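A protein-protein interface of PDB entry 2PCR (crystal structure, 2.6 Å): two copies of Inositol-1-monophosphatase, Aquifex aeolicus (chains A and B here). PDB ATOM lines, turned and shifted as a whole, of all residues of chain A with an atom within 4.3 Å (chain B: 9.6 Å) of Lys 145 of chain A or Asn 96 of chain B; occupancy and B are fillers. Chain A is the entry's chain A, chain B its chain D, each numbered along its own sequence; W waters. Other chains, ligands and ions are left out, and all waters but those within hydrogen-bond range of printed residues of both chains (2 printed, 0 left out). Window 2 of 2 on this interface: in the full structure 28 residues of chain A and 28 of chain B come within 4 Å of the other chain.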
ATOM      1  N   LYS A 143      20.958  24.706  15.946  1.00  0.00           N
ATOM      2  CA  LYS A 143      20.188  25.175  17.092  1.00  0.00           C
ATOM      3  C   LYS A 143      18.851  24.457  17.142  1.00  0.00           C
ATOM      4  O   LYS A 143      18.298  24.093  16.106  1.00  0.00           O
ATOM      5  CB  LYS A 143      19.944  26.685  16.999  1.00  0.00           C
ATOM      6  CG  LYS A 143      19.158  27.144  15.762  1.00  0.00           C
ATOM      7  CD  LYS A 143      18.689  28.589  15.924  1.00  0.00           C
ATOM      8  CE  LYS A 143      17.937  29.104  14.703  1.00  0.00           C
ATOM      9  NZ  LYS A 143      18.846  29.468  13.584  1.00  0.00           N
ATOM     10  N   VAL A 144      18.334  24.249  18.347  1.00  0.00           N
ATOM     11  CA  VAL A 144      17.046  23.590  18.495  1.00  0.00           C
ATOM     12  C   VAL A 144      15.948  24.459  17.891  1.00  0.00           C
ATOM     13  O   VAL A 144      16.173  25.628  17.592  1.00  0.00           O
ATOM     14  CB  VAL A 144      16.717  23.319  19.969  1.00  0.00           C
ATOM     15  CG1 VAL A 144      17.676  22.292  20.514  1.00  0.00           C
ATOM     16  CG2 VAL A 144      16.770  24.621  20.768  1.00  0.00           C
ATOM     17  N   LYS A 145      14.758  23.891  17.724  1.00  0.00           N
ATOM     18  CA  LYS A 145      13.652  24.629  17.124  1.00  0.00           C
ATOM     19  C   LYS A 145      12.733  25.304  18.133  1.00  0.00           C
ATOM     20  O   LYS A 145      12.782  25.020  19.326  1.00  0.00           O
ATOM     21  CB  LYS A 145      12.818  23.706  16.229  1.00  0.00           C
ATOM     22  CG  LYS A 145      12.051  22.638  16.987  1.00  0.00           C
ATOM     23  CD  LYS A 145      11.012  21.986  16.107  1.00  0.00           C
ATOM     24  CE  LYS A 145      11.644  21.270  14.929  1.00  0.00           C
ATOM     25  NZ  LYS A 145      10.634  20.780  13.942  1.00  0.00           N
ATOM     26  N   ASP A 146      11.898  26.206  17.625  1.00  0.00           N
ATOM     27  CA  ASP A 146      10.931  26.943  18.430  1.00  0.00           C
ATOM     28  C   ASP A 146       9.593  26.216  18.354  1.00  0.00           C
ATOM     29  O   ASP A 146       9.276  25.596  17.340  1.00  0.00           O
ATOM     30  CB  ASP A 146      10.736  28.357  17.868  1.00  0.00           C
ATOM     31  CG  ASP A 146      12.029  29.145  17.767  1.00  0.00           C
ATOM     32  OD1 ASP A 146      12.016  30.205  17.106  1.00  0.00           O
ATOM     33  OD2 ASP A 146      13.051  28.723  18.345  1.00  0.00           O
ATOM     34  N   ASN A 147       8.795  26.297  19.410  1.00  0.00           N
ATOM     35  CA  ASN A 147       7.500  25.644  19.378  1.00  0.00           C
ATOM     36  C   ASN A 147       6.406  26.493  19.993  1.00  0.00           C
ATOM     37  O   ASN A 147       6.468  26.852  21.169  1.00  0.00           O
ATOM     38  CB  ASN A 147       7.562  24.298  20.087  1.00  0.00           C
ATOM     39  CG  ASN A 147       6.211  23.621  20.149  1.00  0.00           C
ATOM     40  OD1 ASN A 147       5.434  23.842  21.081  1.00  0.00           O
ATOM     41  ND2 ASN A 147       5.910  22.810  19.137  1.00  0.00           N
ATOM     42  N   GLY A 154       7.328  17.367  17.241  1.00  0.00           N
ATOM     43  CA  GLY A 154       7.725  16.019  16.889  1.00  0.00           C
ATOM     44  C   GLY A 154       8.562  15.510  18.045  1.00  0.00           C
ATOM     45  O   GLY A 154       9.441  16.216  18.535  1.00  0.00           O
ATOM     46  N   SER A 183       3.472  14.283  16.450  1.00  0.00           N
ATOM     47  CA  SER A 183       4.066  12.997  16.124  1.00  0.00           C
ATOM     48  C   SER A 183       5.101  12.485  17.111  1.00  0.00           C
ATOM     49  O   SER A 183       5.739  13.250  17.841  1.00  0.00           O
ATOM     50  CB  SER A 183       4.698  13.043  14.726  1.00  0.00           C
ATOM     51  OG  SER A 183       5.794  13.942  14.684  1.00  0.00           O
ATOM     52  N   GLY A 200      17.338  20.752  15.392  1.00  0.00           N
ATOM     53  CA  GLY A 200      16.016  21.303  15.211  1.00  0.00           C
ATOM     54  C   GLY A 200      15.102  20.482  14.310  1.00  0.00           C
ATOM     55  O   GLY A 200      14.251  21.035  13.617  1.00  0.00           O
ATOM     56  N   ILE A 201      15.280  19.164  14.302  1.00  0.00           N
ATOM     57  CA  ILE A 201      14.427  18.305  13.498  1.00  0.00           C
ATOM     58  C   ILE A 201      13.283  17.854  14.392  1.00  0.00           C
ATOM     59  O   ILE A 201      12.132  17.760  13.959  1.00  0.00           O
ATOM     60  CB  ILE A 201      15.202  17.080  12.953  1.00  0.00           C
ATOM     61  CG1 ILE A 201      16.096  17.528  11.792  1.00  0.00           C
ATOM     62  CG2 ILE A 201      14.236  15.990  12.509  1.00  0.00           C
ATOM     63  CD1 ILE A 201      16.966  16.438  11.232  1.00  0.00           C
ATOM     64  N   PHE A 202      13.607  17.592  15.653  1.00  0.00           N
ATOM     65  CA  PHE A 202      12.607  17.170  16.625  1.00  0.00           C
ATOM     66  C   PHE A 202      12.600  18.118  17.804  1.00  0.00           C
ATOM     67  O   PHE A 202      13.651  18.574  18.244  1.00  0.00           O
ATOM     68  CB  PHE A 202      12.889  15.745  17.105  1.00  0.00           C
ATOM     69  CG  PHE A 202      12.588  14.699  16.078  1.00  0.00           C
ATOM     70  CD1 PHE A 202      11.273  14.455  15.686  1.00  0.00           C
ATOM     71  CD2 PHE A 202      13.616  13.966  15.489  1.00  0.00           C
ATOM     72  CE1 PHE A 202      10.982  13.491  14.717  1.00  0.00           C
ATOM     73  CE2 PHE A 202      13.343  12.999  14.520  1.00  0.00           C
ATOM     74  CZ  PHE A 202      12.021  12.760  14.132  1.00  0.00           C
ATOM     75  N   ASP A 203      11.401  18.412  18.295  1.00  0.00           N
ATOM     76  CA  ASP A 203      11.206  19.302  19.424  1.00  0.00           C
ATOM     77  C   ASP A 203      11.827  18.718  20.685  1.00  0.00           C
ATOM     78  O   ASP A 203      12.264  19.462  21.557  1.00  0.00           O
ATOM     79  CB  ASP A 203       9.706  19.546  19.639  1.00  0.00           C
ATOM     80  CG  ASP A 203       9.079  20.351  18.510  1.00  0.00           C
ATOM     81  OD1 ASP A 203       9.062  21.596  18.619  1.00  0.00           O
ATOM     82  OD2 ASP A 203       8.618  19.750  17.509  1.00  0.00           O
ATOM     83  N   ASN A 245      13.538  21.448  23.150  1.00  0.00           N
ATOM     84  CA  ASN A 245      13.379  22.875  23.345  1.00  0.00           C
ATOM     85  C   ASN A 245      12.611  23.032  24.665  1.00  0.00           C
ATOM     86  O   ASN A 245      12.100  22.055  25.216  1.00  0.00           O
ATOM     87  CB  ASN A 245      12.595  23.492  22.191  1.00  0.00           C
ATOM     88  CG  ASN A 245      11.312  22.748  21.893  1.00  0.00           C
ATOM     89  OD1 ASN A 245      10.577  22.355  22.801  1.00  0.00           O
ATOM     90  ND2 ASN A 245      11.027  22.561  20.613  1.00  0.00           N
ATOM     91  N   ASN B  25      11.604  20.730  -2.538  1.00  0.00           N
ATOM     92  CA  ASN B  25      10.907  21.513  -1.527  1.00  0.00           C
ATOM     93  C   ASN B  25      11.248  21.044  -0.119  1.00  0.00           C
ATOM     94  O   ASN B  25      10.844  21.660   0.865  1.00  0.00           O
ATOM     95  CB  ASN B  25       9.398  21.445  -1.752  1.00  0.00           C
ATOM     96  CG  ASN B  25       8.963  22.184  -3.000  1.00  0.00           C
ATOM     97  OD1 ASN B  25       9.195  23.382  -3.129  1.00  0.00           O
ATOM     98  ND2 ASN B  25       8.328  21.476  -3.923  1.00  0.00           N
ATOM     99  N   PHE B  26      11.993  19.949  -0.023  1.00  0.00           N
ATOM    100  CA  PHE B  26      12.391  19.426   1.275  1.00  0.00           C
ATOM    101  C   PHE B  26      13.311  20.449   1.922  1.00  0.00           C
ATOM    102  O   PHE B  26      14.220  20.961   1.278  1.00  0.00           O
ATOM    103  CB  PHE B  26      13.136  18.098   1.118  1.00  0.00           C
ATOM    104  CG  PHE B  26      13.565  17.487   2.425  1.00  0.00           C
ATOM    105  CD1 PHE B  26      12.620  17.018   3.334  1.00  0.00           C
ATOM    106  CD2 PHE B  26      14.916  17.406   2.758  1.00  0.00           C
ATOM    107  CE1 PHE B  26      13.013  16.477   4.559  1.00  0.00           C
ATOM    108  CE2 PHE B  26      15.321  16.868   3.977  1.00  0.00           C
ATOM    109  CZ  PHE B  26      14.364  16.401   4.882  1.00  0.00           C
ATOM    110  N   GLY B  27      13.080  20.742   3.194  1.00  0.00           N
ATOM    111  CA  GLY B  27      13.909  21.719   3.869  1.00  0.00           C
ATOM    112  C   GLY B  27      13.235  23.075   3.926  1.00  0.00           C
ATOM    113  O   GLY B  27      13.413  23.819   4.889  1.00  0.00           O
ATOM    114  N   LYS B  28      12.464  23.408   2.894  1.00  0.00           N
ATOM    115  CA  LYS B  28      11.758  24.683   2.864  1.00  0.00           C
ATOM    116  C   LYS B  28      10.578  24.600   3.826  1.00  0.00           C
ATOM    117  O   LYS B  28       9.463  24.253   3.430  1.00  0.00           O
ATOM    118  CB  LYS B  28      11.259  24.984   1.450  1.00  0.00           C
ATOM    119  CG  LYS B  28      12.370  25.138   0.428  1.00  0.00           C
ATOM    120  CD  LYS B  28      11.813  25.353  -0.967  1.00  0.00           C
ATOM    121  CE  LYS B  28      12.926  25.415  -2.002  1.00  0.00           C
ATOM    122  NZ  LYS B  28      12.392  25.443  -3.393  1.00  0.00           N
ATOM    123  N   VAL B  29      10.842  24.918   5.093  1.00  0.00           N
ATOM    124  CA  VAL B  29       9.829  24.872   6.144  1.00  0.00           C
ATOM    125  C   VAL B  29       8.427  25.153   5.613  1.00  0.00           C
ATOM    126  O   VAL B  29       7.565  24.262   5.762  1.00  0.00           O
ATOM    127  CB  VAL B  29      10.159  25.868   7.293  1.00  0.00           C
ATOM    128  CG1 VAL B  29      11.490  25.495   7.940  1.00  0.00           C
ATOM    129  CG2 VAL B  29      10.217  27.290   6.760  1.00  0.00           C
ATOM    130  N   PHE B  42       5.929  24.999   1.878  1.00  0.00           N
ATOM    131  CA  PHE B  42       4.587  24.721   2.472  1.00  0.00           C
ATOM    132  C   PHE B  42       4.331  23.211   2.495  1.00  0.00           C
ATOM    133  O   PHE B  42       5.250  22.417   2.280  1.00  0.00           O
ATOM    134  CB  PHE B  42       3.498  25.425   1.653  1.00  0.00           C
ATOM    135  CG  PHE B  42       2.132  25.390   2.288  1.00  0.00           C
ATOM    136  CD1 PHE B  42       0.989  25.372   1.493  1.00  0.00           C
ATOM    137  CD2 PHE B  42       1.985  25.375   3.676  1.00  0.00           C
ATOM    138  CE1 PHE B  42      -0.276  25.342   2.063  1.00  0.00           C
ATOM    139  CE2 PHE B  42       0.721  25.345   4.261  1.00  0.00           C
ATOM    140  CZ  PHE B  42      -0.414  25.328   3.451  1.00  0.00           C
ATOM    141  N   VAL B  43       3.088  22.815   2.759  1.00  0.00           N
ATOM    142  CA  VAL B  43       2.726  21.404   2.811  1.00  0.00           C
ATOM    143  C   VAL B  43       1.604  21.047   1.850  1.00  0.00           C
ATOM    144  O   VAL B  43       1.762  20.166   1.004  1.00  0.00           O
ATOM    145  CB  VAL B  43       2.310  20.989   4.233  1.00  0.00           C
ATOM    146  CG1 VAL B  43       3.528  20.954   5.127  1.00  0.00           C
ATOM    147  CG2 VAL B  43       1.275  21.965   4.785  1.00  0.00           C
ATOM    148  N   LEU B  88       2.415  12.224  -0.728  1.00  0.00           N
ATOM    149  CA  LEU B  88       3.457  12.409   0.265  1.00  0.00           C
ATOM    150  C   LEU B  88       3.209  11.557   1.506  1.00  0.00           C
ATOM    151  O   LEU B  88       2.417  11.929   2.373  1.00  0.00           O
ATOM    152  CB  LEU B  88       3.533  13.883   0.676  1.00  0.00           C
ATOM    153  CG  LEU B  88       4.832  14.426   1.285  1.00  0.00           C
ATOM    154  CD1 LEU B  88       4.571  15.848   1.730  1.00  0.00           C
ATOM    155  CD2 LEU B  88       5.303  13.595   2.464  1.00  0.00           C
ATOM    156  N   GLY B  90       4.488  10.271   4.954  1.00  0.00           N
ATOM    157  CA  GLY B  90       5.481  10.696   5.929  1.00  0.00           C
ATOM    158  C   GLY B  90       5.427  12.206   6.078  1.00  0.00           C
ATOM    159  O   GLY B  90       6.428  12.856   6.384  1.00  0.00           O
ATOM    160  N   THR B  91       4.235  12.751   5.852  1.00  0.00           N
ATOM    161  CA  THR B  91       3.973  14.182   5.930  1.00  0.00           C
ATOM    162  C   THR B  91       4.660  14.868   7.104  1.00  0.00           C
ATOM    163  O   THR B  91       5.474  15.773   6.914  1.00  0.00           O
ATOM    164  CB  THR B  91       2.452  14.456   6.036  1.00  0.00           C
ATOM    165  OG1 THR B  91       1.758  13.730   5.016  1.00  0.00           O
ATOM    166  CG2 THR B  91       2.163  15.943   5.867  1.00  0.00           C
ATOM    167  N   LYS B  92       4.320  14.441   8.315  1.00  0.00           N
ATOM    168  CA  LYS B  92       4.888  15.027   9.517  1.00  0.00           C
ATOM    169  C   LYS B  92       6.403  14.948   9.570  1.00  0.00           C
ATOM    170  O   LYS B  92       7.059  15.859  10.064  1.00  0.00           O
ATOM    171  CB  LYS B  92       4.291  14.372  10.756  1.00  0.00           C
ATOM    172  CG  LYS B  92       2.803  14.587  10.892  1.00  0.00           C
ATOM    173  CD  LYS B  92       2.325  14.248  12.289  1.00  0.00           C
ATOM    174  CE  LYS B  92       0.828  14.457  12.419  1.00  0.00           C
ATOM    175  NZ  LYS B  92       0.470  15.883  12.182  1.00  0.00           N
ATOM    176  N   ASN B  93       6.961  13.851   9.075  1.00  0.00           N
ATOM    177  CA  ASN B  93       8.403  13.696   9.069  1.00  0.00           C
ATOM    178  C   ASN B  93       8.978  14.722   8.093  1.00  0.00           C
ATOM    179  O   ASN B  93       9.964  15.401   8.387  1.00  0.00           O
ATOM    180  CB  ASN B  93       8.784  12.279   8.627  1.00  0.00           C
ATOM    181  CG  ASN B  93       8.568  11.237   9.722  1.00  0.00           C
ATOM    182  OD1 ASN B  93       8.669  10.033   9.474  1.00  0.00           O
ATOM    183  ND2 ASN B  93       8.285  11.697  10.937  1.00  0.00           N
ATOM    184  N   TYR B  94       8.331  14.831   6.940  1.00  0.00           N
ATOM    185  CA  TYR B  94       8.742  15.749   5.882  1.00  0.00           C
ATOM    186  C   TYR B  94       8.787  17.198   6.377  1.00  0.00           C
ATOM    187  O   TYR B  94       9.738  17.928   6.108  1.00  0.00           O
ATOM    188  CB  TYR B  94       7.785  15.599   4.686  1.00  0.00           C
ATOM    189  CG  TYR B  94       8.149  16.427   3.476  1.00  0.00           C
ATOM    190  CD1 TYR B  94       7.593  17.690   3.278  1.00  0.00           C
ATOM    191  CD2 TYR B  94       9.080  15.966   2.551  1.00  0.00           C
ATOM    192  CE1 TYR B  94       7.962  18.477   2.193  1.00  0.00           C
ATOM    193  CE2 TYR B  94       9.457  16.743   1.459  1.00  0.00           C
ATOM    194  CZ  TYR B  94       8.897  18.000   1.284  1.00  0.00           C
ATOM    195  OH  TYR B  94       9.287  18.784   0.220  1.00  0.00           O
ATOM    196  N   ILE B  95       7.760  17.602   7.112  1.00  0.00           N
ATOM    197  CA  ILE B  95       7.677  18.950   7.642  1.00  0.00           C
ATOM    198  C   ILE B  95       8.763  19.195   8.686  1.00  0.00           C
ATOM    199  O   ILE B  95       9.287  20.301   8.813  1.00  0.00           O
ATOM    200  CB  ILE B  95       6.299  19.184   8.295  1.00  0.00           C
ATOM    201  CG1 ILE B  95       5.201  19.070   7.237  1.00  0.00           C
ATOM    202  CG2 ILE B  95       6.244  20.553   8.965  1.00  0.00           C
ATOM    203  CD1 ILE B  95       3.800  19.168   7.814  1.00  0.00           C
ATOM    204  N   ASN B  96       9.099  18.151   9.429  1.00  0.00           N
ATOM    205  CA  ASN B  96      10.106  18.252  10.473  1.00  0.00           C
ATOM    206  C   ASN B  96      11.531  18.179   9.953  1.00  0.00           C
ATOM    207  O   ASN B  96      12.465  18.614  10.622  1.00  0.00           O
ATOM    208  CB  ASN B  96       9.875  17.153  11.500  1.00  0.00           C
ATOM    209  CG  ASN B  96       8.728  17.466  12.421  1.00  0.00           C
ATOM    210  OD1 ASN B  96       8.236  16.596  13.144  1.00  0.00           O
ATOM    211  ND2 ASN B  96       8.301  18.723  12.416  1.00  0.00           N
ATOM    212  N   GLY B  97      11.693  17.635   8.753  1.00  0.00           N
ATOM    213  CA  GLY B  97      13.018  17.512   8.184  1.00  0.00           C
ATOM    214  C   GLY B  97      13.627  16.144   8.410  1.00  0.00           C
ATOM    215  O   GLY B  97      14.817  15.958   8.194  1.00  0.00           O
ATOM    216  N   PHE B  98      12.817  15.187   8.859  1.00  0.00           N
ATOM    217  CA  PHE B  98      13.281  13.814   9.090  1.00  0.00           C
ATOM    218  C   PHE B  98      13.090  13.119   7.738  1.00  0.00           C
ATOM    219  O   PHE B  98      11.963  12.945   7.270  1.00  0.00           O
ATOM    220  CB  PHE B  98      12.445  13.162  10.197  1.00  0.00           C
ATOM    221  CG  PHE B  98      12.916  11.794  10.590  1.00  0.00           C
ATOM    222  CD1 PHE B  98      14.243  11.574  10.951  1.00  0.00           C
ATOM    223  CD2 PHE B  98      12.030  10.718  10.609  1.00  0.00           C
ATOM    224  CE1 PHE B  98      14.681  10.307  11.323  1.00  0.00           C
ATOM    225  CE2 PHE B  98      12.462   9.444  10.983  1.00  0.00           C
ATOM    226  CZ  PHE B  98      13.793   9.238  11.341  1.00  0.00           C
ATOM    227  N   PRO B  99      14.197  12.718   7.093  1.00  0.00           N
ATOM    228  CA  PRO B  99      14.236  12.060   5.780  1.00  0.00           C
ATOM    229  C   PRO B  99      13.371  10.840   5.488  1.00  0.00           C
ATOM    230  O   PRO B  99      13.349  10.374   4.354  1.00  0.00           O
ATOM    231  CB  PRO B  99      15.720  11.766   5.595  1.00  0.00           C
ATOM    232  CG  PRO B  99      16.158  11.462   6.977  1.00  0.00           C
ATOM    233  CD  PRO B  99      15.502  12.583   7.765  1.00  0.00           C
ATOM    234  N   ILE B 100      12.660  10.311   6.476  1.00  0.00           N
ATOM    235  CA  ILE B 100      11.823   9.146   6.204  1.00  0.00           C
ATOM    236  C   ILE B 100      10.475   9.570   5.644  1.00  0.00           C
ATOM    237  O   ILE B 100       9.541   9.861   6.392  1.00  0.00           O
ATOM    238  CB  ILE B 100      11.611   8.272   7.475  1.00  0.00           C
ATOM    239  CG1 ILE B 100      12.917   7.562   7.845  1.00  0.00           C
ATOM    240  CG2 ILE B 100      10.530   7.221   7.225  1.00  0.00           C
ATOM    241  CD1 ILE B 100      13.355   6.508   6.839  1.00  0.00           C
ATOM    242  N   PHE B 101      10.391   9.618   4.318  1.00  0.00           N
ATOM    243  CA  PHE B 101       9.156   9.991   3.628  1.00  0.00           C
ATOM    244  C   PHE B 101       9.187   9.510   2.176  1.00  0.00           C
ATOM    245  O   PHE B 101      10.256   9.247   1.625  1.00  0.00           O
ATOM    246  CB  PHE B 101       8.937  11.513   3.693  1.00  0.00           C
ATOM    247  CG  PHE B 101      10.015  12.316   3.024  1.00  0.00           C
ATOM    248  CD1 PHE B 101       9.956  12.597   1.661  1.00  0.00           C
ATOM    249  CD2 PHE B 101      11.116  12.763   3.752  1.00  0.00           C
ATOM    250  CE1 PHE B 101      10.990  13.315   1.032  1.00  0.00           C
ATOM    251  CE2 PHE B 101      12.147  13.476   3.132  1.00  0.00           C
ATOM    252  CZ  PHE B 101      12.087  13.753   1.777  1.00  0.00           C
ATOM    253  N   PRO B 187       9.441   4.447  12.337  1.00  0.00           N
ATOM    254  CA  PRO B 187       9.915   5.450  11.375  1.00  0.00           C
ATOM    255  C   PRO B 187       8.914   6.550  11.005  1.00  0.00           C
ATOM    256  O   PRO B 187       9.315   7.688  10.773  1.00  0.00           O
ATOM    257  CB  PRO B 187      10.332   4.605  10.179  1.00  0.00           C
ATOM    258  CG  PRO B 187      10.794   3.316  10.846  1.00  0.00           C
ATOM    259  CD  PRO B 187       9.676   3.085  11.829  1.00  0.00           C
HETATM  260  O   HOH W   1       8.050  13.501  12.883  1.00  0.00           O
HETATM  261  O   HOH W   2       4.999  16.526  13.977  1.00  0.00           O
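NZ of Lys 145 of chain A lies close to ND2 of Asn 96 of chain B. The backbone carbonyl oxygen of Ile 201 of chain A sits close to the backbone carbonyl oxygen of Asn 96 of chain B.
The backbone carbonyl oxygen (O) of Lys 92 of chain B lies close to the side-chain amide oxygen (OD1) of Asn 96 of chain B, 3.4 Å away. The side-chain amide nitrogen (ND2) of Asn 245 of chain A lies close to the backbone carbonyl oxygen (O) of Lys 145 of chain A, at 3.3 Å. The side-chain carboxylate (OD2) of Asp 203 of chain A sits at hydrogen-bond distance from the backbone NH (N) of Gly 154 of chain A, at 2.7 Å. O of Ile 201 of chain A is in hydrogen-bond range of NZ of Lys 145 of chain A, 3.4 Å away. O of Asn 93 of chain B sits at hydrogen-bond distance from N of Phe 98 of chain B, at 2.9 Å.
Asn 96 of chain B touches Gly 154 of chain A. Ser 183 of chain A touches Lys 92 of chain B. Asn 96 of chain B touches Ser 183 of chain A. Ile 201 of chain A touches Gly 97 of chain B (CD1 to O, 3.8 Å). N of Phe 98 of chain B touches CG2 of Ile 201 of chain A (3.998 Å). Phe 202 of chain A touches Phe 98 of chain B (CZ to CG, 3.8 Å).
No residue of chain B comes within 4 Å of Val 144 of chain A. Lys 145 of chain A touches just one residue of chain B: Asn 96 (3.5 Å). Of the printed residues of chain B, Gly 154 of chain A touches Asn 96 (3.8 Å). No residue of chain B comes within 4 Å of Gly 200 of chain A. Of the printed residues of chain B, Ile 201 of chain A touches Asn 96, Gly 97 and Phe 98. Of the printed residues of chain B, Phe 202 of chain A touches Phe 98. Gly 27 of chain B touches none of the printed residues of chain A. Printed residues of chain A within 4 Å of Lys 92 of chain B: Ser 183. Printed residues of chain A within 4 Å of Asn 96 of chain B: Lys 145 (3.5 Å), Gly 154 (3.8 Å), Ser 183 (3.9 Å) and Ile 201 (3.4 Å). Of the printed residues of chain A, Gly 97 of chain B touches Ile 201 (3.8 Å). The nearest residue of chain B that does not touch Lys 145 of chain A is Ile 95 of chain B (5.3 Å). The nearest printed residue of chain A that does not touch Gly 97 of chain B is Lys 145 of chain A (6.2 Å).
Of the 12 printed residues of chain A, 5 touch a printed residue of chain B. Printed residues of chain A that touch a printed residue of chain B: Lys 145, Gly 154, Ser 183, Ile 201 and Phe 202. Hydrophobic or aromatic side chains of chain A within 4 Å of the printed part of chain B: Ile 201 and Phe 202. Among the printed residues, 8 pairs touch across the chains. Among the printed residues, no Asp or Glu carboxylate lies within 4 Å of a Lys or Arg side-chain nitrogen of the other chain.
No position is printed for both chains.
Water W1 lies within hydrogen-bond range of ND2 of Asn 93 of chain B (2.7 Å), OG of Ser 183 of chain A (2.9 Å) and OD1 of Asn 96 of chain B (3.1 Å). Water W2 lies within hydrogen-bond range of OG of Ser 183 of chain A (2.8 Å) and OD1 of Asn 96 of chain B (3.3 Å).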
